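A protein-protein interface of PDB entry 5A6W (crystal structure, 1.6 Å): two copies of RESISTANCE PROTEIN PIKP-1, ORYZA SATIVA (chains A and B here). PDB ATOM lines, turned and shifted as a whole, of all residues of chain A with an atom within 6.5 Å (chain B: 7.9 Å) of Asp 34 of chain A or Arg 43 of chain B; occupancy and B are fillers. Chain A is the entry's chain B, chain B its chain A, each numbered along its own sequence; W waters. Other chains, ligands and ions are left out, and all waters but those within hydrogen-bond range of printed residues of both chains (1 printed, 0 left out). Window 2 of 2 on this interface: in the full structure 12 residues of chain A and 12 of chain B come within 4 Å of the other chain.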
ATOM      1  N   LYS A   5      11.724  -7.356  -6.152  1.00  0.00           N
ATOM      2  CA  LYS A   5      12.694  -6.992  -7.129  1.00  0.00           C
ATOM      3  C   LYS A   5      13.376  -8.205  -7.735  1.00  0.00           C
ATOM      4  O   LYS A   5      13.418  -9.306  -7.166  1.00  0.00           O
ATOM      5  CB  LYS A   5      13.785  -6.075  -6.530  1.00  0.00           C
ATOM      6  CG  LYS A   5      13.259  -4.836  -5.807  1.00  0.00           C
ATOM      7  CD  LYS A   5      12.386  -3.986  -6.708  1.00  0.00           C
ATOM      8  CE  LYS A   5      11.620  -2.936  -5.948  1.00  0.00           C
ATOM      9  NZ  LYS A   5      12.479  -1.748  -5.786  1.00  0.00           N
ATOM     10  N   THR A  30      17.284   2.090 -18.380  1.00  0.00           N
ATOM     11  CA  THR A  30      16.154   1.191 -18.588  1.00  0.00           C
ATOM     12  C   THR A  30      15.071   1.357 -17.510  1.00  0.00           C
ATOM     13  O   THR A  30      15.331   1.525 -16.306  1.00  0.00           O
ATOM     14  CB  THR A  30      16.665  -0.254 -18.702  1.00  0.00           C
ATOM     15  OG1 THR A  30      17.596  -0.302 -19.788  1.00  0.00           O
ATOM     16  CG2 THR A  30      15.519  -1.236 -18.978  1.00  0.00           C
ATOM     17  N   GLY A  32      12.476   0.888 -14.743  1.00  0.00           N
ATOM     18  CA  GLY A  32      12.339  -0.047 -13.616  1.00  0.00           C
ATOM     19  C   GLY A  32      13.628  -0.338 -12.883  1.00  0.00           C
ATOM     20  O   GLY A  32      13.602  -1.008 -11.834  1.00  0.00           O
ATOM     21  N   VAL A  33      14.743   0.211 -13.380  1.00  0.00           N
ATOM     22  CA  VAL A  33      16.068  -0.037 -12.765  1.00  0.00           C
ATOM     23  C   VAL A  33      16.273   0.738 -11.470  1.00  0.00           C
ATOM     24  O   VAL A  33      16.101   1.972 -11.412  1.00  0.00           O
ATOM     25  CB  VAL A  33      17.213   0.166 -13.808  1.00  0.00           C
ATOM     26  CG1 VAL A  33      18.597   0.146 -13.163  1.00  0.00           C
ATOM     27  CG2 VAL A  33      17.124  -0.868 -14.894  1.00  0.00           C
ATOM     28  N   ASP A  34      16.608   0.046 -10.399  1.00  0.00           N
ATOM     29  CA  ASP A  34      16.993   0.659  -9.119  1.00  0.00           C
ATOM     30  C   ASP A  34      18.505   0.841  -8.982  1.00  0.00           C
ATOM     31  O   ASP A  34      18.964   1.834  -8.397  1.00  0.00           O
ATOM     32  CB  ASP A  34      16.554  -0.195  -7.942  1.00  0.00           C
ATOM     33  CG  ASP A  34      15.048  -0.351  -7.877  1.00  0.00           C
ATOM     34  OD1 ASP A  34      14.343   0.628  -8.183  1.00  0.00           O
ATOM     35  OD2 ASP A  34      14.615  -1.441  -7.477  1.00  0.00           O
ATOM     36  N   SER A  35      19.286  -0.124  -9.460  1.00  0.00           N
ATOM     37  CA  SER A  35      20.762  -0.065  -9.269  1.00  0.00           C
ATOM     38  C   SER A  35      21.458  -0.941 -10.293  1.00  0.00           C
ATOM     39  O   SER A  35      20.875  -1.907 -10.768  1.00  0.00           O
ATOM     40  CB  SER A  35      21.174  -0.473  -7.843  1.00  0.00           C
ATOM     41  OG  SER A  35      20.652  -1.727  -7.457  1.00  0.00           O
ATOM     42  N   VAL A  36      22.688  -0.578 -10.653  1.00  0.00           N
ATOM     43  CA  VAL A  36      23.503  -1.288 -11.628  1.00  0.00           C
ATOM     44  C   VAL A  36      24.926  -1.283 -11.115  1.00  0.00           C
ATOM     45  O   VAL A  36      25.407  -0.253 -10.608  1.00  0.00           O
ATOM     46  CB  VAL A  36      23.495  -0.535 -12.964  1.00  0.00           C
ATOM     47  CG1 VAL A  36      24.306  -1.264 -14.016  1.00  0.00           C
ATOM     48  CG2 VAL A  36      22.065  -0.303 -13.410  1.00  0.00           C
ATOM     49  N   VAL A  48      22.086  -5.983 -12.426  1.00  0.00           N
ATOM     50  CA  VAL A  48      21.003  -4.996 -12.499  1.00  0.00           C
ATOM     51  C   VAL A  48      19.899  -5.444 -11.544  1.00  0.00           C
ATOM     52  O   VAL A  48      19.475  -6.632 -11.574  1.00  0.00           O
ATOM     53  CB  VAL A  48      20.400  -4.919 -13.911  1.00  0.00           C
ATOM     54  CG1 VAL A  48      19.447  -3.729 -13.988  1.00  0.00           C
ATOM     55  CG2 VAL A  48      21.494  -4.911 -14.965  1.00  0.00           C
ATOM     56  N   VAL A  49      19.405  -4.517 -10.706  1.00  0.00           N
ATOM     57  CA  VAL A  49      18.302  -4.791  -9.791  1.00  0.00           C
ATOM     58  C   VAL A  49      17.198  -3.803 -10.078  1.00  0.00           C
ATOM     59  O   VAL A  49      17.444  -2.640 -10.261  1.00  0.00           O
ATOM     60  CB  VAL A  49      18.759  -4.694  -8.321  1.00  0.00           C
ATOM     61  CG1 VAL A  49      17.572  -4.730  -7.342  1.00  0.00           C
ATOM     62  CG2 VAL A  49      19.750  -5.810  -8.052  1.00  0.00           C
ATOM     63  N   GLY A  50      15.973  -4.297 -10.100  1.00  0.00           N
ATOM     64  CA  GLY A  50      14.824  -3.442 -10.304  1.00  0.00           C
ATOM     65  C   GLY A  50      13.537  -4.223 -10.415  1.00  0.00           C
ATOM     66  O   GLY A  50      13.437  -5.335  -9.968  1.00  0.00           O
ATOM     67  N   TYR A  51      12.563  -3.591 -11.034  1.00  0.00           N
ATOM     68  CA  TYR A  51      11.217  -4.117 -11.157  1.00  0.00           C
ATOM     69  C   TYR A  51      10.703  -3.898 -12.574  1.00  0.00           C
ATOM     70  O   TYR A  51      10.855  -2.827 -13.129  1.00  0.00           O
ATOM     71  CB  TYR A  51      10.305  -3.382 -10.186  1.00  0.00           C
ATOM     72  CG  TYR A  51       8.917  -3.907 -10.210  1.00  0.00           C
ATOM     73  CD1 TYR A  51       8.614  -5.147  -9.642  1.00  0.00           C
ATOM     74  CD2 TYR A  51       7.901  -3.218 -10.875  1.00  0.00           C
ATOM     75  CE1 TYR A  51       7.344  -5.660  -9.692  1.00  0.00           C
ATOM     76  CE2 TYR A  51       6.612  -3.736 -10.929  1.00  0.00           C
ATOM     77  CZ  TYR A  51       6.341  -4.949 -10.309  1.00  0.00           C
ATOM     78  OH  TYR A  51       5.063  -5.499 -10.354  1.00  0.00           O
ATOM     79  N   ILE A  53      11.685  -5.346 -15.346  1.00  0.00           N
ATOM     80  CA  ILE A  53      12.776  -5.389 -16.333  1.00  0.00           C
ATOM     81  C   ILE A  53      12.657  -6.697 -17.119  1.00  0.00           C
ATOM     82  O   ILE A  53      12.450  -7.754 -16.540  1.00  0.00           O
ATOM     83  CB  ILE A  53      14.152  -5.324 -15.669  1.00  0.00           C
ATOM     84  CG1 ILE A  53      14.333  -4.024 -14.875  1.00  0.00           C
ATOM     85  CG2 ILE A  53      15.247  -5.406 -16.744  1.00  0.00           C
ATOM     86  CD1 ILE A  53      15.394  -4.115 -13.801  1.00  0.00           C
ATOM     87  N   ILE B  10      24.558  12.021  -4.227  1.00  0.00           N
ATOM     88  CA  ILE B  10      24.012  13.267  -4.783  1.00  0.00           C
ATOM     89  C   ILE B  10      22.487  13.282  -4.703  1.00  0.00           C
ATOM     90  O   ILE B  10      21.828  12.319  -5.082  1.00  0.00           O
ATOM     91  CB  ILE B  10      24.461  13.460  -6.247  1.00  0.00           C
ATOM     92  CG1 ILE B  10      25.979  13.629  -6.312  1.00  0.00           C
ATOM     93  CG2 ILE B  10      23.831  14.680  -6.861  1.00  0.00           C
ATOM     94  CD1 ILE B  10      26.539  13.540  -7.713  1.00  0.00           C
ATOM     95  N   LYS B  11      21.937  14.379  -4.183  1.00  0.00           N
ATOM     96  CA  LYS B  11      20.482  14.613  -4.210  1.00  0.00           C
ATOM     97  C   LYS B  11      20.163  15.432  -5.446  1.00  0.00           C
ATOM     98  O   LYS B  11      20.840  16.427  -5.728  1.00  0.00           O
ATOM     99  CB  LYS B  11      20.006  15.347  -2.969  1.00  0.00           C
ATOM    100  CG  LYS B  11      18.501  15.490  -2.890  1.00  0.00           C
ATOM    101  CD  LYS B  11      18.101  16.125  -1.575  1.00  0.00           C
ATOM    102  CE  LYS B  11      16.595  16.206  -1.437  1.00  0.00           C
ATOM    103  NZ  LYS B  11      16.204  17.063  -0.286  1.00  0.00           N
ATOM    104  N   VAL B  12      19.160  14.992  -6.206  1.00  0.00           N
ATOM    105  CA  VAL B  12      18.821  15.636  -7.461  1.00  0.00           C
ATOM    106  C   VAL B  12      17.338  15.960  -7.491  1.00  0.00           C
ATOM    107  O   VAL B  12      16.501  15.198  -6.992  1.00  0.00           O
ATOM    108  CB  VAL B  12      19.157  14.750  -8.673  1.00  0.00           C
ATOM    109  CG1 VAL B  12      19.024  15.532  -9.964  1.00  0.00           C
ATOM    110  CG2 VAL B  12      20.560  14.168  -8.560  1.00  0.00           C
ATOM    111  N   MET B  14      14.122  15.798  -9.316  1.00  0.00           N
ATOM    112  CA  MET B  14      13.594  14.855 -10.316  1.00  0.00           C
ATOM    113  C   MET B  14      12.242  15.317 -10.890  1.00  0.00           C
ATOM    114  O   MET B  14      11.320  14.517 -11.045  1.00  0.00           O
ATOM    115  CB  MET B  14      13.423  13.464  -9.681  1.00  0.00           C
ATOM    116  CG  MET B  14      14.675  12.881  -9.030  1.00  0.00           C
ATOM    117  SD  MET B  14      16.036  12.601 -10.191  1.00  0.00           S
ATOM    118  CE  MET B  14      17.027  11.423  -9.272  1.00  0.00           C
ATOM    119  N   ASN B  17       9.838   8.754 -13.561  1.00  0.00           N
ATOM    120  CA  ASN B  17      11.022   7.992 -13.940  1.00  0.00           C
ATOM    121  C   ASN B  17      11.824   8.651 -15.077  1.00  0.00           C
ATOM    122  O   ASN B  17      12.956   8.244 -15.349  1.00  0.00           O
ATOM    123  CB  ASN B  17      10.630   6.554 -14.318  1.00  0.00           C
ATOM    124  CG  ASN B  17      11.780   5.561 -14.152  1.00  0.00           C
ATOM    125  OD1 ASN B  17      12.780   5.846 -13.490  1.00  0.00           O
ATOM    126  ND2 ASN B  17      11.635   4.384 -14.753  1.00  0.00           N
ATOM    127  N   CYS B  19      13.190  11.929 -15.180  1.00  0.00           N
ATOM    128  CA  CYS B  19      14.406  12.558 -14.658  1.00  0.00           C
ATOM    129  C   CYS B  19      15.284  11.538 -13.941  1.00  0.00           C
ATOM    130  O   CYS B  19      16.513  11.646 -13.960  1.00  0.00           O
ATOM    131  CB  CYS B  19      14.076  13.725 -13.726  1.00  0.00           C
ATOM    132  SG  CYS B  19      13.326  15.132 -14.588  1.00  0.00           S
ATOM    133  N   ARG B  20      14.652  10.557 -13.307  1.00  0.00           N
ATOM    134  CA  ARG B  20      15.405   9.524 -12.594  1.00  0.00           C
ATOM    135  C   ARG B  20      16.262   8.697 -13.553  1.00  0.00           C
ATOM    136  O   ARG B  20      17.469   8.531 -13.325  1.00  0.00           O
ATOM    137  CB  ARG B  20      14.475   8.634 -11.768  1.00  0.00           C
ATOM    138  CG  ARG B  20      14.026   9.302 -10.478  1.00  0.00           C
ATOM    139  CD  ARG B  20      12.859   8.572  -9.840  1.00  0.00           C
ATOM    140  NE  ARG B  20      12.367   9.266  -8.651  1.00  0.00           N
ATOM    141  CZ  ARG B  20      11.590  10.357  -8.662  1.00  0.00           C
ATOM    142  NH1 ARG B  20      11.208  10.933  -9.806  1.00  0.00           N
ATOM    143  NH2 ARG B  20      11.197  10.892  -7.511  1.00  0.00           N
ATOM    144  N   SER B  21      15.655   8.192 -14.626  1.00  0.00           N
ATOM    145  CA  SER B  21      16.399   7.398 -15.607  1.00  0.00           C
ATOM    146  C   SER B  21      17.483   8.233 -16.264  1.00  0.00           C
ATOM    147  O   SER B  21      18.613   7.772 -16.450  1.00  0.00           O
ATOM    148  CB  SER B  21      15.480   6.808 -16.671  1.00  0.00           C
ATOM    149  OG  SER B  21      14.628   5.834 -16.101  1.00  0.00           O
ATOM    150  N   MET B  24      20.265   8.698 -13.800  1.00  0.00           N
ATOM    151  CA  MET B  24      20.998   7.448 -13.625  1.00  0.00           C
ATOM    152  C   MET B  24      21.914   7.156 -14.811  1.00  0.00           C
ATOM    153  O   MET B  24      23.047   6.733 -14.640  1.00  0.00           O
ATOM    154  CB  MET B  24      20.018   6.277 -13.422  1.00  0.00           C
ATOM    155  CG  MET B  24      19.363   6.299 -12.050  1.00  0.00           C
ATOM    156  SD  MET B  24      20.459   5.682 -10.764  1.00  0.00           S
ATOM    157  CE  MET B  24      20.218   3.923 -10.987  1.00  0.00           C
ATOM    158  N   VAL B  36      25.938   2.459  -9.632  1.00  0.00           N
ATOM    159  CA  VAL B  36      24.986   3.535  -9.366  1.00  0.00           C
ATOM    160  C   VAL B  36      23.717   2.967  -8.792  1.00  0.00           C
ATOM    161  O   VAL B  36      23.251   1.895  -9.221  1.00  0.00           O
ATOM    162  CB  VAL B  36      24.559   4.335 -10.618  1.00  0.00           C
ATOM    163  CG1 VAL B  36      25.624   5.322 -11.020  1.00  0.00           C
ATOM    164  CG2 VAL B  36      24.155   3.435 -11.783  1.00  0.00           C
ATOM    165  N   ALA B  37      23.136   3.683  -7.830  1.00  0.00           N
ATOM    166  CA  ALA B  37      21.950   3.223  -7.154  1.00  0.00           C
ATOM    167  C   ALA B  37      21.066   4.382  -6.770  1.00  0.00           C
ATOM    168  O   ALA B  37      21.545   5.380  -6.216  1.00  0.00           O
ATOM    169  CB  ALA B  37      22.297   2.390  -5.932  1.00  0.00           C
ATOM    170  N   LEU B  38      19.775   4.225  -7.030  1.00  0.00           N
ATOM    171  CA  LEU B  38      18.770   5.244  -6.745  1.00  0.00           C
ATOM    172  C   LEU B  38      18.239   4.940  -5.384  1.00  0.00           C
ATOM    173  O   LEU B  38      17.644   3.867  -5.194  1.00  0.00           O
ATOM    174  CB  LEU B  38      17.655   5.179  -7.785  1.00  0.00           C
ATOM    175  CG  LEU B  38      16.650   6.301  -7.867  1.00  0.00           C
ATOM    176  CD1 LEU B  38      17.358   7.590  -8.242  1.00  0.00           C
ATOM    177  CD2 LEU B  38      15.590   5.887  -8.882  1.00  0.00           C
ATOM    178  N   VAL B  39      18.404   5.884  -4.438  1.00  0.00           N
ATOM    179  CA  VAL B  39      18.041   5.661  -3.027  1.00  0.00           C
ATOM    180  C   VAL B  39      17.234   6.819  -2.436  1.00  0.00           C
ATOM    181  O   VAL B  39      17.002   7.795  -3.123  1.00  0.00           O
ATOM    182  CB  VAL B  39      19.285   5.423  -2.166  1.00  0.00           C
ATOM    183  CG1 VAL B  39      20.005   4.161  -2.648  1.00  0.00           C
ATOM    184  CG2 VAL B  39      20.208   6.632  -2.173  1.00  0.00           C
ATOM    185  N   GLY B  40      16.815   6.659  -1.174  1.00  0.00           N
ATOM    186  CA  GLY B  40      15.965   7.629  -0.487  1.00  0.00           C
ATOM    187  C   GLY B  40      14.510   7.210  -0.560  1.00  0.00           C
ATOM    188  O   GLY B  40      14.103   6.540  -1.510  1.00  0.00           O
ATOM    189  N   ASP B  41      13.726   7.603   0.446  1.00  0.00           N
ATOM    190  CA  ASP B  41      12.278   7.383   0.443  1.00  0.00           C
ATOM    191  C   ASP B  41      11.584   8.079  -0.725  1.00  0.00           C
ATOM    192  O   ASP B  41      10.529   7.639  -1.154  1.00  0.00           O
ATOM    193  CB  ASP B  41      11.639   7.900   1.731  1.00  0.00           C
ATOM    194  CG  ASP B  41      12.036   7.111   2.957  1.00  0.00           C
ATOM    195  OD1 ASP B  41      12.846   6.177   2.854  1.00  0.00           O
ATOM    196  OD2 ASP B  41      11.518   7.429   4.046  1.00  0.00           O
ATOM    197  N   LEU B  42      12.153   9.177  -1.223  1.00  0.00           N
ATOM    198  CA  LEU B  42      11.595   9.843  -2.404  1.00  0.00           C
ATOM    199  C   LEU B  42      12.306   9.445  -3.680  1.00  0.00           C
ATOM    200  O   LEU B  42      11.979   9.959  -4.751  1.00  0.00           O
ATOM    201  CB  LEU B  42      11.621  11.375  -2.261  1.00  0.00           C
ATOM    202  CG  LEU B  42      10.888  12.053  -1.102  1.00  0.00           C
ATOM    203  CD1 LEU B  42       9.489  11.482  -0.944  1.00  0.00           C
ATOM    204  CD2 LEU B  42      11.680  11.962   0.202  1.00  0.00           C
ATOM    205  N   ARG B  43      13.255   8.511  -3.567  1.00  0.00           N
ATOM    206  CA  ARG B  43      14.028   8.018  -4.709  1.00  0.00           C
ATOM    207  C   ARG B  43      14.616   9.202  -5.478  1.00  0.00           C
ATOM    208  O   ARG B  43      14.484   9.296  -6.699  1.00  0.00           O
ATOM    209  CB  ARG B  43      13.156   7.122  -5.597  1.00  0.00           C
ATOM    210  CG  ARG B  43      12.989   5.709  -5.034  1.00  0.00           C
ATOM    211  CD  ARG B  43      11.854   4.937  -5.701  1.00  0.00           C
ATOM    212  NE  ARG B  43      11.844   5.137  -7.152  1.00  0.00           N
ATOM    213  CZ  ARG B  43      12.511   4.406  -8.049  1.00  0.00           C
ATOM    214  NH1 ARG B  43      13.273   3.358  -7.696  1.00  0.00           N
ATOM    215  NH2 ARG B  43      12.403   4.735  -9.336  1.00  0.00           N
ATOM    216  N   ASP B  44      15.227  10.126  -4.734  1.00  0.00           N
ATOM    217  CA  ASP B  44      15.780  11.353  -5.321  1.00  0.00           C
ATOM    218  C   ASP B  44      17.275  11.512  -5.069  1.00  0.00           C
ATOM    219  O   ASP B  44      17.836  12.590  -5.310  1.00  0.00           O
ATOM    220  CB  ASP B  44      15.038  12.595  -4.800  1.00  0.00           C
ATOM    221  CG  ASP B  44      15.129  12.776  -3.279  1.00  0.00           C
ATOM    222  OD1 ASP B  44      15.500  11.828  -2.556  1.00  0.00           O
ATOM    223  OD2 ASP B  44      14.777  13.900  -2.804  1.00  0.00           O
ATOM    224  N   LYS B  45      17.922  10.451  -4.597  1.00  0.00           N
ATOM    225  CA  LYS B  45      19.363  10.466  -4.338  1.00  0.00           C
ATOM    226  C   LYS B  45      20.007   9.372  -5.158  1.00  0.00           C
ATOM    227  O   LYS B  45      19.412   8.308  -5.349  1.00  0.00           O
ATOM    228  CB  LYS B  45      19.665  10.222  -2.860  1.00  0.00           C
ATOM    229  CG  LYS B  45      19.156  11.367  -1.988  1.00  0.00           C
ATOM    230  CD  LYS B  45      19.092  11.020  -0.506  1.00  0.00           C
ATOM    231  CE  LYS B  45      18.390  12.151   0.225  1.00  0.00           C
ATOM    232  NZ  LYS B  45      18.008  11.860   1.632  1.00  0.00           N
ATOM    233  N   ILE B  46      21.223   9.628  -5.601  1.00  0.00           N
ATOM    234  CA  ILE B  46      21.986   8.644  -6.363  1.00  0.00           C
ATOM    235  C   ILE B  46      23.308   8.442  -5.651  1.00  0.00           C
ATOM    236  O   ILE B  46      24.021   9.408  -5.362  1.00  0.00           O
ATOM    237  CB  ILE B  46      22.239   9.091  -7.802  1.00  0.00           C
ATOM    238  CG1 ILE B  46      20.902   9.248  -8.542  1.00  0.00           C
ATOM    239  CG2 ILE B  46      23.097   8.050  -8.534  1.00  0.00           C
ATOM    240  CD1 ILE B  46      21.067   9.849  -9.923  1.00  0.00           C
ATOM    241  N   GLU B  47      23.593   7.172  -5.354  1.00  0.00           N
ATOM    242  CA  GLU B  47      24.859   6.714  -4.788  1.00  0.00           C
ATOM    243  C   GLU B  47      25.714   6.217  -5.923  1.00  0.00           C
ATOM    244  O   GLU B  47      25.281   5.342  -6.713  1.00  0.00           O
ATOM    245  CB  GLU B  47      24.663   5.569  -3.781  1.00  0.00           C
ATOM    246  CG  GLU B  47      23.732   5.901  -2.616  1.00  0.00           C
ATOM    247  CD  GLU B  47      23.640   4.823  -1.560  1.00  0.00           C
ATOM    248  OE1 GLU B  47      24.178   3.710  -1.775  1.00  0.00           O
ATOM    249  OE2 GLU B  47      23.015   5.093  -0.488  1.00  0.00           O
HETATM  250  O   HOH W   1      16.284   3.846 -15.399  1.00  0.00           O
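Hydrophobic or aromatic side chains of chain B that line the printed part of chain A: Met 24, Ala 37 and Leu 38. Printed residues of chain A that touch a printed residue of chain B: Gly 32, Asp 34, Ser 35 and Val 36. Among the printed residues, 8 pairs touch across the chains.
N of Leu 38 of chain B sits at hydrogen-bond distance from O of Asp 34 of chain A (2.9 Å). The backbone NH (N) of Val 36 of chain A is in hydrogen-bond range of the backbone carbonyl oxygen (O) of Val 36 of chain B (2.9 Å). The guanidinium group of Arg 43 of chain B is in salt-bridge range of the side-chain carboxylate of Asp 34 of chain A (3.0 Å).
Asp 34 of chain A touches just these residues of chain B: Met 24, Ala 37, Leu 38 and Arg 43. Arg 43 of chain B touches just one residue of chain A: Asp 34 (3.0 Å). Printed residues of chain A within 4 Å of Ala 37 of chain B: Asp 34 and Ser 35. Printed residues of chain A within 4 Å of Met 24 of chain B: Asp 34. Of the printed residues of chain B, Gly 32 of chain A touches Asn 17 (3.6 Å). Printed residues of chain A within 4 Å of Val 36 of chain B: Ser 35 (3.2 Å) and Val 36 (2.9 Å). Printed residues of chain A within 4 Å of Leu 38 of chain B: Asp 34 (2.9 Å). Ile 46 of chain B touches none of the printed residues of chain A.
NZ of Lys 5 of chain A lies within salt-bridge range of OD2 of Asp 34 of chain A (2.7 Å). O of Asn 17 of chain B sits at hydrogen-bond distance from OG of Ser 21 of chain B (3.0 Å). The backbone NH (N) of Glu 47 of chain B is in hydrogen-bond range of the backbone carbonyl oxygen (O) of Ala 37 of chain B (2.9 Å). The backbone NH (N) of Tyr 51 of chain A lies within hydrogen-bond range of the backbone carbonyl oxygen (O) of Gly 32 of chain A, at 2.9 Å. O of Ser 35 of chain A sits at hydrogen-bond distance from N of Val 49 of chain A, at 3.0 Å. The backbone carbonyl oxygen of Val 49 of chain A is in hydrogen-bond range of the backbone NH of Asp 34 of chain A.
Among the printed residues, pairs that only touch across the chains: Gly 32 of chain A with Asn 17 of chain B (3.6 Å), Asp 34 of chain A with Met 24 of chain B (3.6 Å), Asp 34 of chain A with Ala 37 of chain B (3.5 Å), Ser 35 of chain A with Val 36 of chain B (3.2 Å) and Ser 35 of chain A with Ala 37 of chain B (3.6 Å).
Val 36 of chain B touches its own counterpart, Val 36 of chain A.
Water W1 lies within hydrogen-bond range of the backbone carbonyl oxygen of Thr 30 of chain A and the side-chain hydroxyl of Ser 21 of chain B.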
